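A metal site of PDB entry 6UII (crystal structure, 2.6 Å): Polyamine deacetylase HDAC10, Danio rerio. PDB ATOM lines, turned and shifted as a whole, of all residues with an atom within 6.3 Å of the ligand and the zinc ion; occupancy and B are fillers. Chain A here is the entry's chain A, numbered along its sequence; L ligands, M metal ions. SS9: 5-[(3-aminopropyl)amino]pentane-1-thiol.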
ATOM      1  N   PRO A  23      29.167  14.139 -16.685  1.00  0.00           N
ATOM      2  CA  PRO A  23      28.182  15.203 -16.940  1.00  0.00           C
ATOM      3  C   PRO A  23      28.551  16.119 -18.091  1.00  0.00           C
ATOM      4  O   PRO A  23      27.666  16.808 -18.619  1.00  0.00           O
ATOM      5  CB  PRO A  23      28.130  15.956 -15.605  1.00  0.00           C
ATOM      6  CG  PRO A  23      28.676  14.982 -14.582  1.00  0.00           C
ATOM      7  CD  PRO A  23      29.716  14.198 -15.318  1.00  0.00           C
ATOM      8  N   ALA A  24      29.818  16.143 -18.501  1.00  0.00           N
ATOM      9  CA  ALA A  24      30.208  17.010 -19.606  1.00  0.00           C
ATOM     10  C   ALA A  24      29.724  16.503 -20.963  1.00  0.00           C
ATOM     11  O   ALA A  24      29.446  17.312 -21.856  1.00  0.00           O
ATOM     12  CB  ALA A  24      31.735  17.173 -19.634  1.00  0.00           C
ATOM     13  N   CYS A  25      29.638  15.182 -21.158  1.00  0.00           N
ATOM     14  CA  CYS A  25      29.303  14.630 -22.471  1.00  0.00           C
ATOM     15  C   CYS A  25      27.981  13.892 -22.521  1.00  0.00           C
ATOM     16  O   CYS A  25      27.633  13.354 -23.590  1.00  0.00           O
ATOM     17  CB  CYS A  25      30.416  13.697 -22.977  1.00  0.00           C
ATOM     18  SG  CYS A  25      32.116  14.203 -22.649  1.00  0.00           S
ATOM     19  N   ILE A  27      25.054  14.982 -22.843  1.00  0.00           N
ATOM     20  CA  ILE A  27      24.088  15.540 -23.769  1.00  0.00           C
ATOM     21  C   ILE A  27      24.307  15.060 -25.202  1.00  0.00           C
ATOM     22  O   ILE A  27      23.388  15.185 -26.026  1.00  0.00           O
ATOM     23  CB  ILE A  27      24.101  17.083 -23.701  1.00  0.00           C
ATOM     24  CG1 ILE A  27      25.405  17.629 -24.268  1.00  0.00           C
ATOM     25  CG2 ILE A  27      23.917  17.542 -22.272  1.00  0.00           C
ATOM     26  CD1 ILE A  27      25.378  19.112 -24.520  1.00  0.00           C
ATOM     27  N   GLU A  28      25.475  14.518 -25.520  1.00  0.00           N
ATOM     28  CA  GLU A  28      25.812  14.127 -26.901  1.00  0.00           C
ATOM     29  C   GLU A  28      25.498  12.645 -27.100  1.00  0.00           C
ATOM     30  O   GLU A  28      26.284  11.778 -26.709  1.00  0.00           O
ATOM     31  CB  GLU A  28      27.271  14.437 -27.200  1.00  0.00           C
ATOM     32  CG  GLU A  28      27.519  14.879 -28.636  1.00  0.00           C
ATOM     33  CD  GLU A  28      27.415  13.733 -29.617  1.00  0.00           C
ATOM     34  OE1 GLU A  28      28.139  12.738 -29.446  1.00  0.00           O
ATOM     35  OE2 GLU A  28      26.593  13.839 -30.562  1.00  0.00           O
ATOM     36  N   ASP A  94      36.479  17.486 -22.604  1.00  0.00           N
ATOM     37  CA  ASP A  94      35.058  17.334 -22.897  1.00  0.00           C
ATOM     38  C   ASP A  94      34.827  16.530 -24.187  1.00  0.00           C
ATOM     39  O   ASP A  94      34.140  16.972 -25.113  1.00  0.00           O
ATOM     40  CB  ASP A  94      34.364  18.705 -22.969  1.00  0.00           C
ATOM     41  CG  ASP A  94      34.166  19.315 -21.604  1.00  0.00           C
ATOM     42  OD1 ASP A  94      34.401  18.634 -20.583  1.00  0.00           O
ATOM     43  OD2 ASP A  94      33.763  20.493 -21.548  1.00  0.00           O
ATOM     44  N   PRO A 134      30.673  15.652 -34.195  1.00  0.00           N
ATOM     45  CA  PRO A 134      30.875  16.993 -34.754  1.00  0.00           C
ATOM     46  C   PRO A 134      32.342  17.259 -35.054  1.00  0.00           C
ATOM     47  O   PRO A 134      33.204  16.411 -34.791  1.00  0.00           O
ATOM     48  CB  PRO A 134      30.357  17.920 -33.650  1.00  0.00           C
ATOM     49  CG  PRO A 134      29.503  17.059 -32.783  1.00  0.00           C
ATOM     50  CD  PRO A 134      30.141  15.715 -32.826  1.00  0.00           C
ATOM     51  N   HIS A 136      33.836  21.123 -35.403  1.00  0.00           N
ATOM     52  CA  HIS A 136      34.430  22.457 -35.407  1.00  0.00           C
ATOM     53  C   HIS A 136      35.334  22.743 -34.216  1.00  0.00           C
ATOM     54  O   HIS A 136      36.093  23.704 -34.267  1.00  0.00           O
ATOM     55  CB  HIS A 136      33.338  23.532 -35.510  1.00  0.00           C
ATOM     56  CG  HIS A 136      32.404  23.582 -34.345  1.00  0.00           C
ATOM     57  ND1 HIS A 136      31.478  24.595 -34.185  1.00  0.00           N
ATOM     58  CD2 HIS A 136      32.226  22.744 -33.300  1.00  0.00           C
ATOM     59  CE1 HIS A 136      30.766  24.369 -33.101  1.00  0.00           C
ATOM     60  NE2 HIS A 136      31.200  23.252 -32.534  1.00  0.00           N
ATOM     61  N   HIS A 137      35.289  21.928 -33.173  1.00  0.00           N
ATOM     62  CA  HIS A 137      36.152  22.121 -32.012  1.00  0.00           C
ATOM     63  C   HIS A 137      37.483  21.393 -32.131  1.00  0.00           C
ATOM     64  O   HIS A 137      38.439  21.780 -31.445  1.00  0.00           O
ATOM     65  CB  HIS A 137      35.445  21.642 -30.745  1.00  0.00           C
ATOM     66  CG  HIS A 137      34.233  22.438 -30.384  1.00  0.00           C
ATOM     67  ND1 HIS A 137      34.230  23.819 -30.400  1.00  0.00           N
ATOM     68  CD2 HIS A 137      32.997  22.050 -30.019  1.00  0.00           C
ATOM     69  CE1 HIS A 137      33.032  24.245 -30.042  1.00  0.00           C
ATOM     70  NE2 HIS A 137      32.267  23.201 -29.802  1.00  0.00           N
ATOM     71  N   GLY A 145      35.621  18.860 -27.293  1.00  0.00           N
ATOM     72  CA  GLY A 145      34.213  19.194 -27.360  1.00  0.00           C
ATOM     73  C   GLY A 145      33.415  18.301 -28.289  1.00  0.00           C
ATOM     74  O   GLY A 145      32.811  18.790 -29.261  1.00  0.00           O
ATOM     75  N   PHE A 146      33.426  17.000 -28.020  1.00  0.00           N
ATOM     76  CA  PHE A 146      32.714  15.944 -28.750  1.00  0.00           C
ATOM     77  C   PHE A 146      33.266  15.718 -30.156  1.00  0.00           C
ATOM     78  O   PHE A 146      32.741  14.856 -30.868  1.00  0.00           O
ATOM     79  CB  PHE A 146      31.199  16.217 -28.860  1.00  0.00           C
ATOM     80  CG  PHE A 146      30.544  16.621 -27.559  1.00  0.00           C
ATOM     81  CD1 PHE A 146      31.041  16.183 -26.344  1.00  0.00           C
ATOM     82  CD2 PHE A 146      29.431  17.450 -27.558  1.00  0.00           C
ATOM     83  CE1 PHE A 146      30.439  16.561 -25.159  1.00  0.00           C
ATOM     84  CE2 PHE A 146      28.826  17.818 -26.364  1.00  0.00           C
ATOM     85  CZ  PHE A 146      29.332  17.379 -25.169  1.00  0.00           C
ATOM     86  N   CYS A 147      34.312  16.436 -30.573  1.00  0.00           N
ATOM     87  CA  CYS A 147      34.818  16.391 -31.939  1.00  0.00           C
ATOM     88  C   CYS A 147      36.106  15.571 -32.006  1.00  0.00           C
ATOM     89  O   CYS A 147      36.974  15.712 -31.139  1.00  0.00           O
ATOM     90  CB  CYS A 147      35.104  17.790 -32.464  1.00  0.00           C
ATOM     91  SG  CYS A 147      33.702  18.927 -32.406  1.00  0.00           S
ATOM     92  N   ASP A 174      26.605  27.501 -34.990  1.00  0.00           N
ATOM     93  CA  ASP A 174      26.554  26.791 -33.711  1.00  0.00           C
ATOM     94  C   ASP A 174      26.757  27.791 -32.563  1.00  0.00           C
ATOM     95  O   ASP A 174      27.385  28.845 -32.729  1.00  0.00           O
ATOM     96  CB  ASP A 174      27.632  25.700 -33.697  1.00  0.00           C
ATOM     97  CG  ASP A 174      27.502  24.764 -32.519  1.00  0.00           C
ATOM     98  OD1 ASP A 174      27.031  23.622 -32.702  1.00  0.00           O
ATOM     99  OD2 ASP A 174      27.881  25.146 -31.407  1.00  0.00           O
ATOM    100  N   VAL A 175      26.200  27.455 -31.385  1.00  0.00           N
ATOM    101  CA  VAL A 175      26.311  28.358 -30.231  1.00  0.00           C
ATOM    102  C   VAL A 175      27.690  28.323 -29.589  1.00  0.00           C
ATOM    103  O   VAL A 175      28.014  29.226 -28.807  1.00  0.00           O
ATOM    104  CB  VAL A 175      25.237  28.023 -29.176  1.00  0.00           C
ATOM    105  CG1 VAL A 175      25.713  26.913 -28.221  1.00  0.00           C
ATOM    106  CG2 VAL A 175      24.826  29.274 -28.394  1.00  0.00           C
ATOM    107  N   HIS A 176      28.510  27.323 -29.889  1.00  0.00           N
ATOM    108  CA  HIS A 176      29.879  27.271 -29.407  1.00  0.00           C
ATOM    109  C   HIS A 176      30.825  27.812 -30.473  1.00  0.00           C
ATOM    110  O   HIS A 176      30.512  27.849 -31.669  1.00  0.00           O
ATOM    111  CB  HIS A 176      30.292  25.848 -29.049  1.00  0.00           C
ATOM    112  CG  HIS A 176      29.428  25.208 -28.023  1.00  0.00           C
ATOM    113  ND1 HIS A 176      28.167  24.715 -28.302  1.00  0.00           N
ATOM    114  CD2 HIS A 176      29.640  24.972 -26.704  1.00  0.00           C
ATOM    115  CE1 HIS A 176      27.642  24.202 -27.204  1.00  0.00           C
ATOM    116  NE2 HIS A 176      28.515  24.351 -26.216  1.00  0.00           N
ATOM    117  N   HIS A 177      32.006  28.225 -30.019  1.00  0.00           N
ATOM    118  CA  HIS A 177      33.019  28.788 -30.910  1.00  0.00           C
ATOM    119  C   HIS A 177      33.781  27.659 -31.591  1.00  0.00           C
ATOM    120  O   HIS A 177      34.280  26.753 -30.914  1.00  0.00           O
ATOM    121  CB  HIS A 177      33.957  29.712 -30.145  1.00  0.00           C
ATOM    122  CG  HIS A 177      35.021  30.332 -31.010  1.00  0.00           C
ATOM    123  ND1 HIS A 177      36.363  30.227 -30.728  1.00  0.00           N
ATOM    124  CD2 HIS A 177      34.932  31.053 -32.154  1.00  0.00           C
ATOM    125  CE1 HIS A 177      37.056  30.855 -31.657  1.00  0.00           C
ATOM    126  NE2 HIS A 177      36.206  31.367 -32.536  1.00  0.00           N
ATOM    127  N   PHE A 204      31.990  31.250 -20.524  1.00  0.00           N
ATOM    128  CA  PHE A 204      31.381  30.069 -21.118  1.00  0.00           C
ATOM    129  C   PHE A 204      32.379  29.287 -21.960  1.00  0.00           C
ATOM    130  O   PHE A 204      33.261  29.857 -22.618  1.00  0.00           O
ATOM    131  CB  PHE A 204      30.175  30.438 -21.977  1.00  0.00           C
ATOM    132  CG  PHE A 204      29.361  29.255 -22.410  1.00  0.00           C
ATOM    133  CD1 PHE A 204      28.616  28.527 -21.489  1.00  0.00           C
ATOM    134  CD2 PHE A 204      29.369  28.839 -23.741  1.00  0.00           C
ATOM    135  CE1 PHE A 204      27.892  27.421 -21.888  1.00  0.00           C
ATOM    136  CE2 PHE A 204      28.646  27.733 -24.130  1.00  0.00           C
ATOM    137  CZ  PHE A 204      27.908  27.024 -23.199  1.00  0.00           C
ATOM    138  N   TRP A 205      32.219  27.956 -21.938  1.00  0.00           N
ATOM    139  CA  TRP A 205      33.116  27.027 -22.615  1.00  0.00           C
ATOM    140  C   TRP A 205      33.227  27.385 -24.101  1.00  0.00           C
ATOM    141  O   TRP A 205      32.224  27.723 -24.739  1.00  0.00           O
ATOM    142  CB  TRP A 205      32.594  25.596 -22.441  1.00  0.00           C
ATOM    143  CG  TRP A 205      33.565  24.539 -22.847  1.00  0.00           C
ATOM    144  CD1 TRP A 205      34.423  23.868 -22.025  1.00  0.00           C
ATOM    145  CD2 TRP A 205      33.777  24.030 -24.170  1.00  0.00           C
ATOM    146  NE1 TRP A 205      35.170  22.985 -22.767  1.00  0.00           N
ATOM    147  CE2 TRP A 205      34.795  23.062 -24.076  1.00  0.00           C
ATOM    148  CE3 TRP A 205      33.208  24.312 -25.414  1.00  0.00           C
ATOM    149  CZ2 TRP A 205      35.253  22.362 -25.197  1.00  0.00           C
ATOM    150  CZ3 TRP A 205      33.670  23.621 -26.524  1.00  0.00           C
ATOM    151  CH2 TRP A 205      34.681  22.654 -26.400  1.00  0.00           C
ATOM    152  N   GLY A 265      25.170  24.105 -36.249  1.00  0.00           N
ATOM    153  CA  GLY A 265      24.776  23.604 -34.942  1.00  0.00           C
ATOM    154  C   GLY A 265      23.455  24.245 -34.566  1.00  0.00           C
ATOM    155  O   GLY A 265      23.261  25.444 -34.780  1.00  0.00           O
ATOM    156  N   ASP A 267      22.176  23.923 -31.380  1.00  0.00           N
ATOM    157  CA  ASP A 267      22.210  24.316 -29.984  1.00  0.00           C
ATOM    158  C   ASP A 267      22.089  25.826 -29.804  1.00  0.00           C
ATOM    159  O   ASP A 267      22.087  26.292 -28.653  1.00  0.00           O
ATOM    160  CB  ASP A 267      23.495  23.818 -29.307  1.00  0.00           C
ATOM    161  CG  ASP A 267      24.745  24.130 -30.108  1.00  0.00           C
ATOM    162  OD1 ASP A 267      24.681  24.937 -31.061  1.00  0.00           O
ATOM    163  OD2 ASP A 267      25.796  23.570 -29.783  1.00  0.00           O
ATOM    164  N   GLU A 274      22.243  23.846 -23.651  1.00  0.00           N
ATOM    165  CA  GLU A 274      23.631  24.281 -23.687  1.00  0.00           C
ATOM    166  C   GLU A 274      23.803  25.724 -24.130  1.00  0.00           C
ATOM    167  O   GLU A 274      24.740  26.379 -23.695  1.00  0.00           O
ATOM    168  CB  GLU A 274      24.432  23.361 -24.616  1.00  0.00           C
ATOM    169  CG  GLU A 274      25.920  23.546 -24.580  1.00  0.00           C
ATOM    170  CD  GLU A 274      26.588  22.942 -23.366  1.00  0.00           C
ATOM    171  OE1 GLU A 274      27.747  23.310 -23.092  1.00  0.00           O
ATOM    172  OE2 GLU A 274      25.946  22.110 -22.669  1.00  0.00           O
ATOM    173  N   GLU A 304      26.570  20.096 -36.630  1.00  0.00           N
ATOM    174  CA  GLU A 304      27.507  20.173 -35.520  1.00  0.00           C
ATOM    175  C   GLU A 304      26.737  19.797 -34.254  1.00  0.00           C
ATOM    176  O   GLU A 304      26.430  18.614 -34.051  1.00  0.00           O
ATOM    177  CB  GLU A 304      28.147  21.556 -35.426  1.00  0.00           C
ATOM    178  CG  GLU A 304      28.915  21.986 -36.670  1.00  0.00           C
ATOM    179  CD  GLU A 304      30.325  21.400 -36.752  1.00  0.00           C
ATOM    180  OE1 GLU A 304      31.024  21.724 -37.742  1.00  0.00           O
ATOM    181  OE2 GLU A 304      30.733  20.636 -35.850  1.00  0.00           O
ATOM    182  N   GLY A 305      26.425  20.756 -33.390  1.00  0.00           N
ATOM    183  CA  GLY A 305      25.685  20.496 -32.172  1.00  0.00           C
ATOM    184  C   GLY A 305      24.197  20.730 -32.316  1.00  0.00           C
ATOM    185  O   GLY A 305      23.669  20.988 -33.404  1.00  0.00           O
ATOM    186  N   GLY A 306      23.509  20.664 -31.168  1.00  0.00           N
ATOM    187  CA  GLY A 306      22.056  20.655 -31.071  1.00  0.00           C
ATOM    188  C   GLY A 306      21.625  19.467 -30.235  1.00  0.00           C
ATOM    189  O   GLY A 306      21.639  18.335 -30.734  1.00  0.00           O
ATOM    190  N   PHE A 307      21.257  19.689 -28.967  1.00  0.00           N
ATOM    191  CA  PHE A 307      21.162  18.597 -28.008  1.00  0.00           C
ATOM    192  C   PHE A 307      19.800  18.455 -27.351  1.00  0.00           C
ATOM    193  O   PHE A 307      19.640  17.591 -26.469  1.00  0.00           O
ATOM    194  CB  PHE A 307      22.249  18.764 -26.929  1.00  0.00           C
ATOM    195  CG  PHE A 307      23.603  18.992 -27.502  1.00  0.00           C
ATOM    196  CD1 PHE A 307      24.409  17.923 -27.843  1.00  0.00           C
ATOM    197  CD2 PHE A 307      24.065  20.285 -27.745  1.00  0.00           C
ATOM    198  CE1 PHE A 307      25.654  18.131 -28.396  1.00  0.00           C
ATOM    199  CE2 PHE A 307      25.311  20.493 -28.288  1.00  0.00           C
ATOM    200  CZ  PHE A 307      26.105  19.416 -28.619  1.00  0.00           C
HETATM  201  C2  SS9 L   1      29.234  20.206 -21.040  1.00  0.00           C
HETATM  202  C3  SS9 L   1      29.797  21.323 -21.911  1.00  0.00           C
HETATM  203  C4  SS9 L   1      30.933  20.793 -22.769  1.00  0.00           C
HETATM  204  C6  SS9 L   1      31.076  20.632 -25.169  1.00  0.00           C
HETATM  205  C7  SS9 L   1      30.931  21.422 -26.447  1.00  0.00           C
HETATM  206  C8  SS9 L   1      29.706  20.950 -27.151  1.00  0.00           C
HETATM  207  C9  SS9 L   1      29.527  21.720 -28.395  1.00  0.00           C
HETATM  208  C10 SS9 L   1      29.387  20.783 -29.528  1.00  0.00           C
HETATM  209  N1  SS9 L   1      28.087  20.573 -20.206  1.00  0.00           N
HETATM  210  N5  SS9 L   1      30.966  21.539 -24.025  1.00  0.00           N
HETATM  211  S11 SS9 L   1      29.005  21.834 -30.915  1.00  0.00           S
HETATM  212 ZN    ZN M   1      27.754  23.613 -30.167  1.00  0.00          ZN
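Ala 24 touches the ligand (O to C2, 3.0 Å).
Gly 145 touches the ligand.
Phe 146 touches the ligand (CE2 to C8, 3.3 Å).
CZ3 of Trp 205 touches C7 of the ligand (3.5 Å).
Phe 307 touches the ligand.
13 residues have an atom within 4 Å of the ligand: Ala 24, Asp 94, His 136, His 137, Gly 145, Phe 146, Asp 174, His 176, Trp 205, Asp 267, Glu 274, Gly 305 and Phe 307.
The nearest printed residue that does not touch the ligand is Pro 23 (4.1 Å).
NE2 of His 136 lies close to S11 of the ligand (3.1 Å).
The side-chain carboxylate (OE2) of Glu 274 is in salt-bridge range of a nitrogen (N1) of the ligand.
N5 of the ligand is in salt-bridge range of OD2 of Asp 94 (3.9 Å).
NE2 of His 137 sits close to S11 of the ligand (3.7 Å).
The backbone NH (N) of Gly 305 lies close to a sulfur (S11) of the ligand (3.7 Å).
The side-chain carboxylate of Asp 267 sits at hydrogen-bond distance from the backbone NH of Val 175.
A ring nitrogen (NE2) of His 136 sits at hydrogen-bond distance from a ring nitrogen (NE2) of His 137, 2.9 Å away.
The side-chain carboxylate (OE2) of Glu 304 sits at hydrogen-bond distance from the backbone NH (N) of His 136, 3.2 Å away.
The backbone NH of His 136 lies within hydrogen-bond range of the side-chain sulfur of Cys 147 (3.7 Å).
The backbone carbonyl oxygen of Asp 94 lies close to the backbone NH of Gly 145 (3.2 Å).
The backbone NH of His 137 sits at hydrogen-bond distance from the side-chain sulfur of Cys 147 (3.5 Å).
The backbone carbonyl oxygen (O) of His 177 sits close to a ring nitrogen (ND1) of His 137 (3.0 Å).
O of Gly 145 lies within hydrogen-bond range of SG of Cys 147.
The zinc ion is bound by the side-chain carboxylate of Asp 174 (2.0 Å), the side-chain carboxylate of Asp 267 (2.0 Å), a ring nitrogen (ND1) of His 176 (2.2 Å) and a sulfur (S11) of the ligand (2.3 Å).
The zinc ion has four donor atoms within binding distance.
Slightly farther from the zinc ion lies the side-chain carboxylate (OD1) of Asp 174 (2.6 Å).
Within 4 Å of the zinc ion: Asp 174, His 176 and Asp 267.
Along chain A the residues within 4 Å of the zinc ion span positions 174 to 267.
The nearest printed residue that does not touch the zinc ion is His 136 (4.2 Å).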
